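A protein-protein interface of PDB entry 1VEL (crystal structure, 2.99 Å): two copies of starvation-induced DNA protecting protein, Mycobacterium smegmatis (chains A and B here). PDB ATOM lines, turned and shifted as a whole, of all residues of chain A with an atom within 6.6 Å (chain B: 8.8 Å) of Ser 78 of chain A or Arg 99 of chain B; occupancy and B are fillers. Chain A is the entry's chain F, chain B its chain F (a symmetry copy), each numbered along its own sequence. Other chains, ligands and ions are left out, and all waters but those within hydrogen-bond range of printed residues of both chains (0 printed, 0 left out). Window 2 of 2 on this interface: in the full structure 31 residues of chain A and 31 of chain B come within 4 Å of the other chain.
The guanidinium group (NH2) of Arg 99 of chain B lies within hydrogen-bond range of the backbone carbonyl oxygen (O) of Gly 76 of chain A (2.5 Å).
The side-chain hydroxyl (OG) of Ser 78 of chain A sits at hydrogen-bond distance from the side-chain amide oxygen (OD1) of Asn 41 of chain B.
The backbone carbonyl oxygen (O) of Pro 79 of chain A sits at hydrogen-bond distance from the side-chain amide nitrogen (ND2) of Asn 41 of chain B.
The side-chain amino group (NZ) of Lys 80 of chain A lies within salt-bridge range of the side-chain carboxylate (OE2) of Glu 98 of chain B.
The backbone NH (N) of Lys 80 of chain A is in hydrogen-bond range of the side-chain amide oxygen (OE1) of Gln 22 of chain A, at 3.0 Å.
The backbone carbonyl oxygen (O) of Ile 72 of chain A is in hydrogen-bond range of the backbone NH (N) of Lys 77 of chain A.
OG of Ser 78 of chain A sits at hydrogen-bond distance from NZ of Lys 80 of chain A, 3.5 Å away.
The backbone carbonyl oxygen (O) of His 37 of chain B sits at hydrogen-bond distance from the side-chain amide nitrogen (ND2) of Asn 41 of chain B (2.9 Å).
O of Val 97 of chain B sits at hydrogen-bond distance from NE2 of His 37 of chain B, 3.1 Å away.
The backbone carbonyl oxygen of Glu 98 of chain B lies within hydrogen-bond range of a ring nitrogen (NE2) of His 105 of chain B (2.8 Å).
Trp 40 of chain B touches Ala 69 of chain A.
Lys 77 of chain A touches Arg 99 of chain B.
Arg 99 of chain B touches Ser 78 of chain A.
O of Pro 79 of chain A touches CE1 of His 37 of chain B (3.5 Å).
His 37 of chain B touches Lys 80 of chain A.
Printed residues of chain B within 4 Å of Ala 69 of chain A: Trp 40 (3.4 Å).
Printed residues of chain B within 4 Å of Gly 76 of chain A: Arg 99 (2.5 Å).
Of chain B, only His 37 and Asn 41 come within 4 Å of Pro 79 of chain A.
Val 38 of chain B touches none of the printed residues of chain A.
Printed residues of chain A within 4 Å of Glu 98 of chain B: Lys 80.
Arg 99 of chain B touches just these residues of chain A: Gly 76, Lys 77 and Ser 78.
The nearest residue of chain B that does not touch Ser 78 of chain A is Glu 98 of chain B (4.03 Å).
The nearest residue of chain A that does not touch Arg 99 of chain B is Phe 4 of chain A (5.1 Å).
The nearest printed residue of chain A that does not touch Glu 98 of chain B is Ser 78 of chain A (4.03 Å).
Hydrophobic or aromatic side chains of chain A within 4 Å of the printed part of chain B: Ala 69 and Pro 79.
Among the printed residues, Asp or Glu carboxylates within 4 Å of a Lys or Arg side-chain nitrogen of the other chain: Lys 80 of chain A with Glu 98 of chain B.
No position is printed for both chains.
Of the 9 pairs that touch across the chains among the printed residues, none has its exchanged pair printed and touching as well.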
ATOM      1  N   SER A   3      -0.281  -3.709 -17.541  1.00  0.00           N
ATOM      2  CA  SER A   3       1.172  -3.400 -17.421  1.00  0.00           C
ATOM      3  C   SER A   3       1.999  -4.665 -17.215  1.00  0.00           C
ATOM      4  O   SER A   3       3.158  -4.592 -16.801  1.00  0.00           O
ATOM      5  CB  SER A   3       1.402  -2.445 -16.265  1.00  0.00           C
ATOM      6  N   PHE A   4       1.395  -5.819 -17.497  1.00  0.00           N
ATOM      7  CA  PHE A   4       2.066  -7.110 -17.361  1.00  0.00           C
ATOM      8  C   PHE A   4       1.295  -8.156 -18.157  1.00  0.00           C
ATOM      9  O   PHE A   4       0.103  -7.994 -18.414  1.00  0.00           O
ATOM     10  CB  PHE A   4       2.130  -7.538 -15.888  1.00  0.00           C
ATOM     11  CG  PHE A   4       0.842  -8.122 -15.364  1.00  0.00           C
ATOM     12  CD1 PHE A   4       0.470  -9.427 -15.679  1.00  0.00           C
ATOM     13  CD2 PHE A   4      -0.010  -7.363 -14.575  1.00  0.00           C
ATOM     14  CE1 PHE A   4      -0.731  -9.960 -15.224  1.00  0.00           C
ATOM     15  CE2 PHE A   4      -1.212  -7.888 -14.116  1.00  0.00           C
ATOM     16  CZ  PHE A   4      -1.570  -9.188 -14.441  1.00  0.00           C
ATOM     17  N   GLN A  22     -12.505 -12.161 -25.010  1.00  0.00           N
ATOM     18  CA  GLN A  22     -13.585 -11.356 -24.435  1.00  0.00           C
ATOM     19  C   GLN A  22     -14.884 -11.489 -25.217  1.00  0.00           C
ATOM     20  O   GLN A  22     -15.975 -11.452 -24.647  1.00  0.00           O
ATOM     21  CB  GLN A  22     -13.185  -9.885 -24.389  1.00  0.00           C
ATOM     22  CG  GLN A  22     -14.324  -8.936 -24.019  1.00  0.00           C
ATOM     23  CD  GLN A  22     -14.831  -9.126 -22.603  1.00  0.00           C
ATOM     24  OE1 GLN A  22     -14.064  -9.077 -21.639  1.00  0.00           O
ATOM     25  NE2 GLN A  22     -16.135  -9.330 -22.469  1.00  0.00           N
ATOM     26  N   ALA A  69     -12.603 -16.127 -18.999  1.00  0.00           N
ATOM     27  CA  ALA A  69     -12.477 -14.885 -18.253  1.00  0.00           C
ATOM     28  C   ALA A  69     -11.164 -14.852 -17.490  1.00  0.00           C
ATOM     29  O   ALA A  69     -10.365 -13.935 -17.659  1.00  0.00           O
ATOM     30  CB  ALA A  69     -13.638 -14.731 -17.285  1.00  0.00           C
ATOM     31  N   ILE A  72      -8.292 -14.181 -19.608  1.00  0.00           N
ATOM     32  CA  ILE A  72      -8.204 -12.791 -20.016  1.00  0.00           C
ATOM     33  C   ILE A  72      -7.531 -11.957 -18.937  1.00  0.00           C
ATOM     34  O   ILE A  72      -6.868 -10.964 -19.222  1.00  0.00           O
ATOM     35  CB  ILE A  72      -9.595 -12.190 -20.236  1.00  0.00           C
ATOM     36  CG1 ILE A  72     -10.268 -12.839 -21.446  1.00  0.00           C
ATOM     37  CG2 ILE A  72      -9.477 -10.681 -20.388  1.00  0.00           C
ATOM     38  CD1 ILE A  72     -11.659 -12.303 -21.716  1.00  0.00           C
ATOM     39  N   ALA A  73      -7.737 -12.356 -17.691  1.00  0.00           N
ATOM     40  CA  ALA A  73      -7.160 -11.658 -16.556  1.00  0.00           C
ATOM     41  C   ALA A  73      -5.677 -11.984 -16.444  1.00  0.00           C
ATOM     42  O   ALA A  73      -4.870 -11.133 -16.074  1.00  0.00           O
ATOM     43  CB  ALA A  73      -7.883 -12.067 -15.294  1.00  0.00           C
ATOM     44  N   GLY A  76      -3.411 -10.130 -18.678  1.00  0.00           N
ATOM     45  CA  GLY A  76      -3.197  -8.739 -18.314  1.00  0.00           C
ATOM     46  C   GLY A  76      -4.370  -7.771 -18.367  1.00  0.00           C
ATOM     47  O   GLY A  76      -4.396  -6.790 -17.625  1.00  0.00           O
ATOM     48  N   LYS A  77      -5.340  -8.025 -19.233  1.00  0.00           N
ATOM     49  CA  LYS A  77      -6.474  -7.127 -19.341  1.00  0.00           C
ATOM     50  C   LYS A  77      -7.534  -7.466 -18.292  1.00  0.00           C
ATOM     51  O   LYS A  77      -7.262  -8.219 -17.359  1.00  0.00           O
ATOM     52  CB  LYS A  77      -7.027  -7.195 -20.763  1.00  0.00           C
ATOM     53  CG  LYS A  77      -5.951  -6.978 -21.845  1.00  0.00           C
ATOM     54  CD  LYS A  77      -5.321  -5.579 -21.772  1.00  0.00           C
ATOM     55  CE  LYS A  77      -4.217  -5.367 -22.812  1.00  0.00           C
ATOM     56  NZ  LYS A  77      -3.030  -6.255 -22.594  1.00  0.00           N
ATOM     57  N   SER A  78      -8.736  -6.912 -18.435  1.00  0.00           N
ATOM     58  CA  SER A  78      -9.815  -7.144 -17.472  1.00  0.00           C
ATOM     59  C   SER A  78     -11.082  -7.666 -18.147  1.00  0.00           C
ATOM     60  O   SER A  78     -11.579  -7.062 -19.093  1.00  0.00           O
ATOM     61  CB  SER A  78     -10.108  -5.837 -16.731  1.00  0.00           C
ATOM     62  OG  SER A  78     -11.465  -5.733 -16.370  1.00  0.00           O
ATOM     63  N   PRO A  79     -11.628  -8.795 -17.661  1.00  0.00           N
ATOM     64  CA  PRO A  79     -12.842  -9.376 -18.249  1.00  0.00           C
ATOM     65  C   PRO A  79     -14.103  -8.634 -17.852  1.00  0.00           C
ATOM     66  O   PRO A  79     -14.252  -8.220 -16.704  1.00  0.00           O
ATOM     67  CB  PRO A  79     -12.851 -10.806 -17.701  1.00  0.00           C
ATOM     68  CG  PRO A  79     -11.448 -11.023 -17.192  1.00  0.00           C
ATOM     69  CD  PRO A  79     -11.091  -9.686 -16.625  1.00  0.00           C
ATOM     70  N   LYS A  80     -15.010  -8.469 -18.807  1.00  0.00           N
ATOM     71  CA  LYS A  80     -16.276  -7.804 -18.538  1.00  0.00           C
ATOM     72  C   LYS A  80     -17.342  -8.880 -18.536  1.00  0.00           C
ATOM     73  O   LYS A  80     -17.585  -9.519 -19.563  1.00  0.00           O
ATOM     74  CB  LYS A  80     -16.589  -6.762 -19.613  1.00  0.00           C
ATOM     75  CG  LYS A  80     -15.832  -5.446 -19.460  1.00  0.00           C
ATOM     76  CD  LYS A  80     -14.351  -5.604 -19.754  1.00  0.00           C
ATOM     77  CE  LYS A  80     -13.616  -4.277 -19.638  1.00  0.00           C
ATOM     78  NZ  LYS A  80     -13.600  -3.761 -18.242  1.00  0.00           N
ATOM     79  N   HIS B  37     -18.313 -11.549 -12.055  1.00  0.00           N
ATOM     80  CA  HIS B  37     -17.581 -10.416 -12.604  1.00  0.00           C
ATOM     81  C   HIS B  37     -16.586  -9.870 -11.588  1.00  0.00           C
ATOM     82  O   HIS B  37     -15.434  -9.619 -11.929  1.00  0.00           O
ATOM     83  CB  HIS B  37     -18.541  -9.301 -13.013  1.00  0.00           C
ATOM     84  CG  HIS B  37     -17.852  -8.064 -13.496  1.00  0.00           C
ATOM     85  ND1 HIS B  37     -17.493  -7.878 -14.813  1.00  0.00           N
ATOM     86  CD2 HIS B  37     -17.418  -6.968 -12.827  1.00  0.00           C
ATOM     87  CE1 HIS B  37     -16.868  -6.720 -14.934  1.00  0.00           C
ATOM     88  NE2 HIS B  37     -16.808  -6.149 -13.744  1.00  0.00           N
ATOM     89  N   VAL B  38     -17.021  -9.672 -10.345  1.00  0.00           N
ATOM     90  CA  VAL B  38     -16.103  -9.161  -9.339  1.00  0.00           C
ATOM     91  C   VAL B  38     -15.210 -10.316  -8.880  1.00  0.00           C
ATOM     92  O   VAL B  38     -14.181 -10.109  -8.240  1.00  0.00           O
ATOM     93  CB  VAL B  38     -16.848  -8.497  -8.130  1.00  0.00           C
ATOM     94  CG1 VAL B  38     -18.301  -8.272  -8.467  1.00  0.00           C
ATOM     95  CG2 VAL B  38     -16.699  -9.318  -6.883  1.00  0.00           C
ATOM     96  N   TRP B  40     -13.654 -12.290 -10.964  1.00  0.00           N
ATOM     97  CA  TRP B  40     -12.492 -12.221 -11.841  1.00  0.00           C
ATOM     98  C   TRP B  40     -11.670 -10.955 -11.731  1.00  0.00           C
ATOM     99  O   TRP B  40     -10.461 -10.992 -11.968  1.00  0.00           O
ATOM    100  CB  TRP B  40     -12.903 -12.371 -13.315  1.00  0.00           C
ATOM    101  CG  TRP B  40     -13.839 -13.502 -13.602  1.00  0.00           C
ATOM    102  CD1 TRP B  40     -13.759 -14.780 -13.119  1.00  0.00           C
ATOM    103  CD2 TRP B  40     -14.990 -13.465 -14.448  1.00  0.00           C
ATOM    104  NE1 TRP B  40     -14.790 -15.538 -13.612  1.00  0.00           N
ATOM    105  CE2 TRP B  40     -15.564 -14.760 -14.430  1.00  0.00           C
ATOM    106  CE3 TRP B  40     -15.594 -12.467 -15.221  1.00  0.00           C
ATOM    107  CZ2 TRP B  40     -16.716 -15.083 -15.155  1.00  0.00           C
ATOM    108  CZ3 TRP B  40     -16.741 -12.789 -15.945  1.00  0.00           C
ATOM    109  CH2 TRP B  40     -17.289 -14.089 -15.904  1.00  0.00           C
ATOM    110  N   ASN B  41     -12.320  -9.846 -11.370  1.00  0.00           N
ATOM    111  CA  ASN B  41     -11.656  -8.539 -11.305  1.00  0.00           C
ATOM    112  C   ASN B  41     -11.087  -8.029  -9.992  1.00  0.00           C
ATOM    113  O   ASN B  41     -10.584  -6.914  -9.929  1.00  0.00           O
ATOM    114  CB  ASN B  41     -12.591  -7.476 -11.890  1.00  0.00           C
ATOM    115  CG  ASN B  41     -12.768  -7.630 -13.393  1.00  0.00           C
ATOM    116  OD1 ASN B  41     -11.805  -7.519 -14.152  1.00  0.00           O
ATOM    117  ND2 ASN B  41     -13.998  -7.896 -13.829  1.00  0.00           N
ATOM    118  N   VAL B  42     -11.155  -8.835  -8.947  1.00  0.00           N
ATOM    119  CA  VAL B  42     -10.634  -8.422  -7.656  1.00  0.00           C
ATOM    120  C   VAL B  42      -9.112  -8.591  -7.588  1.00  0.00           C
ATOM    121  O   VAL B  42      -8.563  -9.561  -8.117  1.00  0.00           O
ATOM    122  CB  VAL B  42     -11.315  -9.230  -6.526  1.00  0.00           C
ATOM    123  CG1 VAL B  42     -10.542  -9.109  -5.248  1.00  0.00           C
ATOM    124  CG2 VAL B  42     -12.714  -8.716  -6.304  1.00  0.00           C
ATOM    125  N   VAL B  43      -8.442  -7.624  -6.959  1.00  0.00           N
ATOM    126  CA  VAL B  43      -6.987  -7.638  -6.775  1.00  0.00           C
ATOM    127  C   VAL B  43      -6.714  -7.161  -5.361  1.00  0.00           C
ATOM    128  O   VAL B  43      -7.556  -6.498  -4.755  1.00  0.00           O
ATOM    129  CB  VAL B  43      -6.244  -6.678  -7.738  1.00  0.00           C
ATOM    130  CG1 VAL B  43      -6.580  -7.007  -9.170  1.00  0.00           C
ATOM    131  CG2 VAL B  43      -6.603  -5.239  -7.424  1.00  0.00           C
ATOM    132  N   GLY B  44      -5.539  -7.495  -4.843  1.00  0.00           N
ATOM    133  CA  GLY B  44      -5.195  -7.080  -3.501  1.00  0.00           C
ATOM    134  C   GLY B  44      -4.556  -8.180  -2.692  1.00  0.00           C
ATOM    135  O   GLY B  44      -4.451  -9.312  -3.148  1.00  0.00           O
ATOM    136  N   TYR B  95     -23.170  -2.983 -12.997  1.00  0.00           N
ATOM    137  CA  TYR B  95     -22.042  -2.846 -12.068  1.00  0.00           C
ATOM    138  C   TYR B  95     -20.914  -2.114 -12.797  1.00  0.00           C
ATOM    139  O   TYR B  95     -20.422  -2.596 -13.817  1.00  0.00           O
ATOM    140  CB  TYR B  95     -21.575  -4.234 -11.613  1.00  0.00           C
ATOM    141  CG  TYR B  95     -20.618  -4.254 -10.439  1.00  0.00           C
ATOM    142  CD1 TYR B  95     -21.056  -3.977  -9.147  1.00  0.00           C
ATOM    143  CD2 TYR B  95     -19.280  -4.593 -10.620  1.00  0.00           C
ATOM    144  CE1 TYR B  95     -20.181  -4.045  -8.063  1.00  0.00           C
ATOM    145  CE2 TYR B  95     -18.403  -4.663  -9.553  1.00  0.00           C
ATOM    146  CZ  TYR B  95     -18.853  -4.390  -8.278  1.00  0.00           C
ATOM    147  OH  TYR B  95     -17.974  -4.474  -7.223  1.00  0.00           O
ATOM    148  N   SER B  96     -20.502  -0.962 -12.270  1.00  0.00           N
ATOM    149  CA  SER B  96     -19.470  -0.152 -12.914  1.00  0.00           C
ATOM    150  C   SER B  96     -18.028  -0.328 -12.479  1.00  0.00           C
ATOM    151  O   SER B  96     -17.165   0.431 -12.915  1.00  0.00           O
ATOM    152  CB  SER B  96     -19.820   1.330 -12.794  1.00  0.00           C
ATOM    153  OG  SER B  96     -20.849   1.683 -13.696  1.00  0.00           O
ATOM    154  N   VAL B  97     -17.749  -1.313 -11.639  1.00  0.00           N
ATOM    155  CA  VAL B  97     -16.380  -1.516 -11.178  1.00  0.00           C
ATOM    156  C   VAL B  97     -15.631  -2.590 -11.965  1.00  0.00           C
ATOM    157  O   VAL B  97     -15.972  -3.774 -11.893  1.00  0.00           O
ATOM    158  CB  VAL B  97     -16.352  -1.904  -9.690  1.00  0.00           C
ATOM    159  CG1 VAL B  97     -14.930  -1.922  -9.181  1.00  0.00           C
ATOM    160  CG2 VAL B  97     -17.167  -0.938  -8.900  1.00  0.00           C
ATOM    161  N   GLU B  98     -14.614  -2.181 -12.724  1.00  0.00           N
ATOM    162  CA  GLU B  98     -13.824  -3.139 -13.491  1.00  0.00           C
ATOM    163  C   GLU B  98     -12.787  -3.666 -12.512  1.00  0.00           C
ATOM    164  O   GLU B  98     -13.113  -3.928 -11.350  1.00  0.00           O
ATOM    165  CB  GLU B  98     -13.113  -2.473 -14.675  1.00  0.00           C
ATOM    166  CG  GLU B  98     -13.961  -1.521 -15.493  1.00  0.00           C
ATOM    167  CD  GLU B  98     -15.400  -1.968 -15.616  1.00  0.00           C
ATOM    168  OE1 GLU B  98     -16.170  -1.765 -14.655  1.00  0.00           O
ATOM    169  OE2 GLU B  98     -15.763  -2.528 -16.667  1.00  0.00           O
ATOM    170  N   ARG B  99     -11.544  -3.804 -12.966  1.00  0.00           N
ATOM    171  CA  ARG B  99     -10.475  -4.289 -12.096  1.00  0.00           C
ATOM    172  C   ARG B  99     -10.186  -3.289 -10.983  1.00  0.00           C
ATOM    173  O   ARG B  99      -9.781  -2.163 -11.252  1.00  0.00           O
ATOM    174  CB  ARG B  99      -9.185  -4.510 -12.879  1.00  0.00           C
ATOM    175  CG  ARG B  99      -8.019  -4.842 -11.960  1.00  0.00           C
ATOM    176  CD  ARG B  99      -6.698  -4.387 -12.528  1.00  0.00           C
ATOM    177  NE  ARG B  99      -6.237  -5.231 -13.627  1.00  0.00           N
ATOM    178  CZ  ARG B  99      -5.931  -4.779 -14.841  1.00  0.00           C
ATOM    179  NH1 ARG B  99      -6.044  -3.486 -15.117  1.00  0.00           N
ATOM    180  NH2 ARG B  99      -5.507  -5.619 -15.775  1.00  0.00           N
ATOM    181  N   ASP B 100     -10.375  -3.697  -9.737  1.00  0.00           N
ATOM    182  CA  ASP B 100     -10.113  -2.791  -8.631  1.00  0.00           C
ATOM    183  C   ASP B 100      -9.753  -3.596  -7.395  1.00  0.00           C
ATOM    184  O   ASP B 100      -9.579  -4.808  -7.478  1.00  0.00           O
ATOM    185  CB  ASP B 100     -11.340  -1.922  -8.359  1.00  0.00           C
ATOM    186  CG  ASP B 100     -10.977  -0.495  -7.986  1.00  0.00           C
ATOM    187  OD1 ASP B 100     -10.178  -0.294  -7.045  1.00  0.00           O
ATOM    188  OD2 ASP B 100     -11.505   0.426  -8.638  1.00  0.00           O
ATOM    189  N   THR B 101      -9.648  -2.924  -6.252  1.00  0.00           N
ATOM    190  CA  THR B 101      -9.283  -3.597  -5.011  1.00  0.00           C
ATOM    191  C   THR B 101     -10.431  -4.408  -4.435  1.00  0.00           C
ATOM    192  O   THR B 101     -11.573  -4.279  -4.865  1.00  0.00           O
ATOM    193  CB  THR B 101      -8.832  -2.590  -3.939  1.00  0.00           C
ATOM    194  OG1 THR B 101      -9.952  -1.812  -3.507  1.00  0.00           O
ATOM    195  CG2 THR B 101      -7.784  -1.661  -4.497  1.00  0.00           C
ATOM    196  N   VAL B 102     -10.110  -5.252  -3.460  1.00  0.00           N
ATOM    197  CA  VAL B 102     -11.106  -6.075  -2.789  1.00  0.00           C
ATOM    198  C   VAL B 102     -12.044  -5.143  -2.038  1.00  0.00           C
ATOM    199  O   VAL B 102     -13.263  -5.298  -2.084  1.00  0.00           O
ATOM    200  CB  VAL B 102     -10.448  -7.033  -1.775  1.00  0.00           C
ATOM    201  CG1 VAL B 102     -11.513  -7.782  -0.987  1.00  0.00           C
ATOM    202  CG2 VAL B 102      -9.543  -8.007  -2.497  1.00  0.00           C
ATOM    203  N   ALA B 104     -12.756  -2.115  -2.698  1.00  0.00           N
ATOM    204  CA  ALA B 104     -13.572  -1.387  -3.673  1.00  0.00           C
ATOM    205  C   ALA B 104     -14.817  -2.165  -4.085  1.00  0.00           C
ATOM    206  O   ALA B 104     -15.944  -1.671  -3.994  1.00  0.00           O
ATOM    207  CB  ALA B 104     -12.745  -1.074  -4.903  1.00  0.00           C
ATOM    208  N   HIS B 105     -14.587  -3.382  -4.560  1.00  0.00           N
ATOM    209  CA  HIS B 105     -15.648  -4.271  -4.999  1.00  0.00           C
ATOM    210  C   HIS B 105     -16.608  -4.625  -3.877  1.00  0.00           C
ATOM    211  O   HIS B 105     -17.819  -4.597  -4.064  1.00  0.00           O
ATOM    212  CB  HIS B 105     -15.040  -5.542  -5.585  1.00  0.00           C
ATOM    213  CG  HIS B 105     -14.598  -5.393  -7.002  1.00  0.00           C
ATOM    214  ND1 HIS B 105     -15.488  -5.343  -8.053  1.00  0.00           N
ATOM    215  CD2 HIS B 105     -13.366  -5.255  -7.545  1.00  0.00           C
ATOM    216  CE1 HIS B 105     -14.821  -5.182  -9.183  1.00  0.00           C
ATOM    217  NE2 HIS B 105     -13.532  -5.124  -8.902  1.00  0.00           N
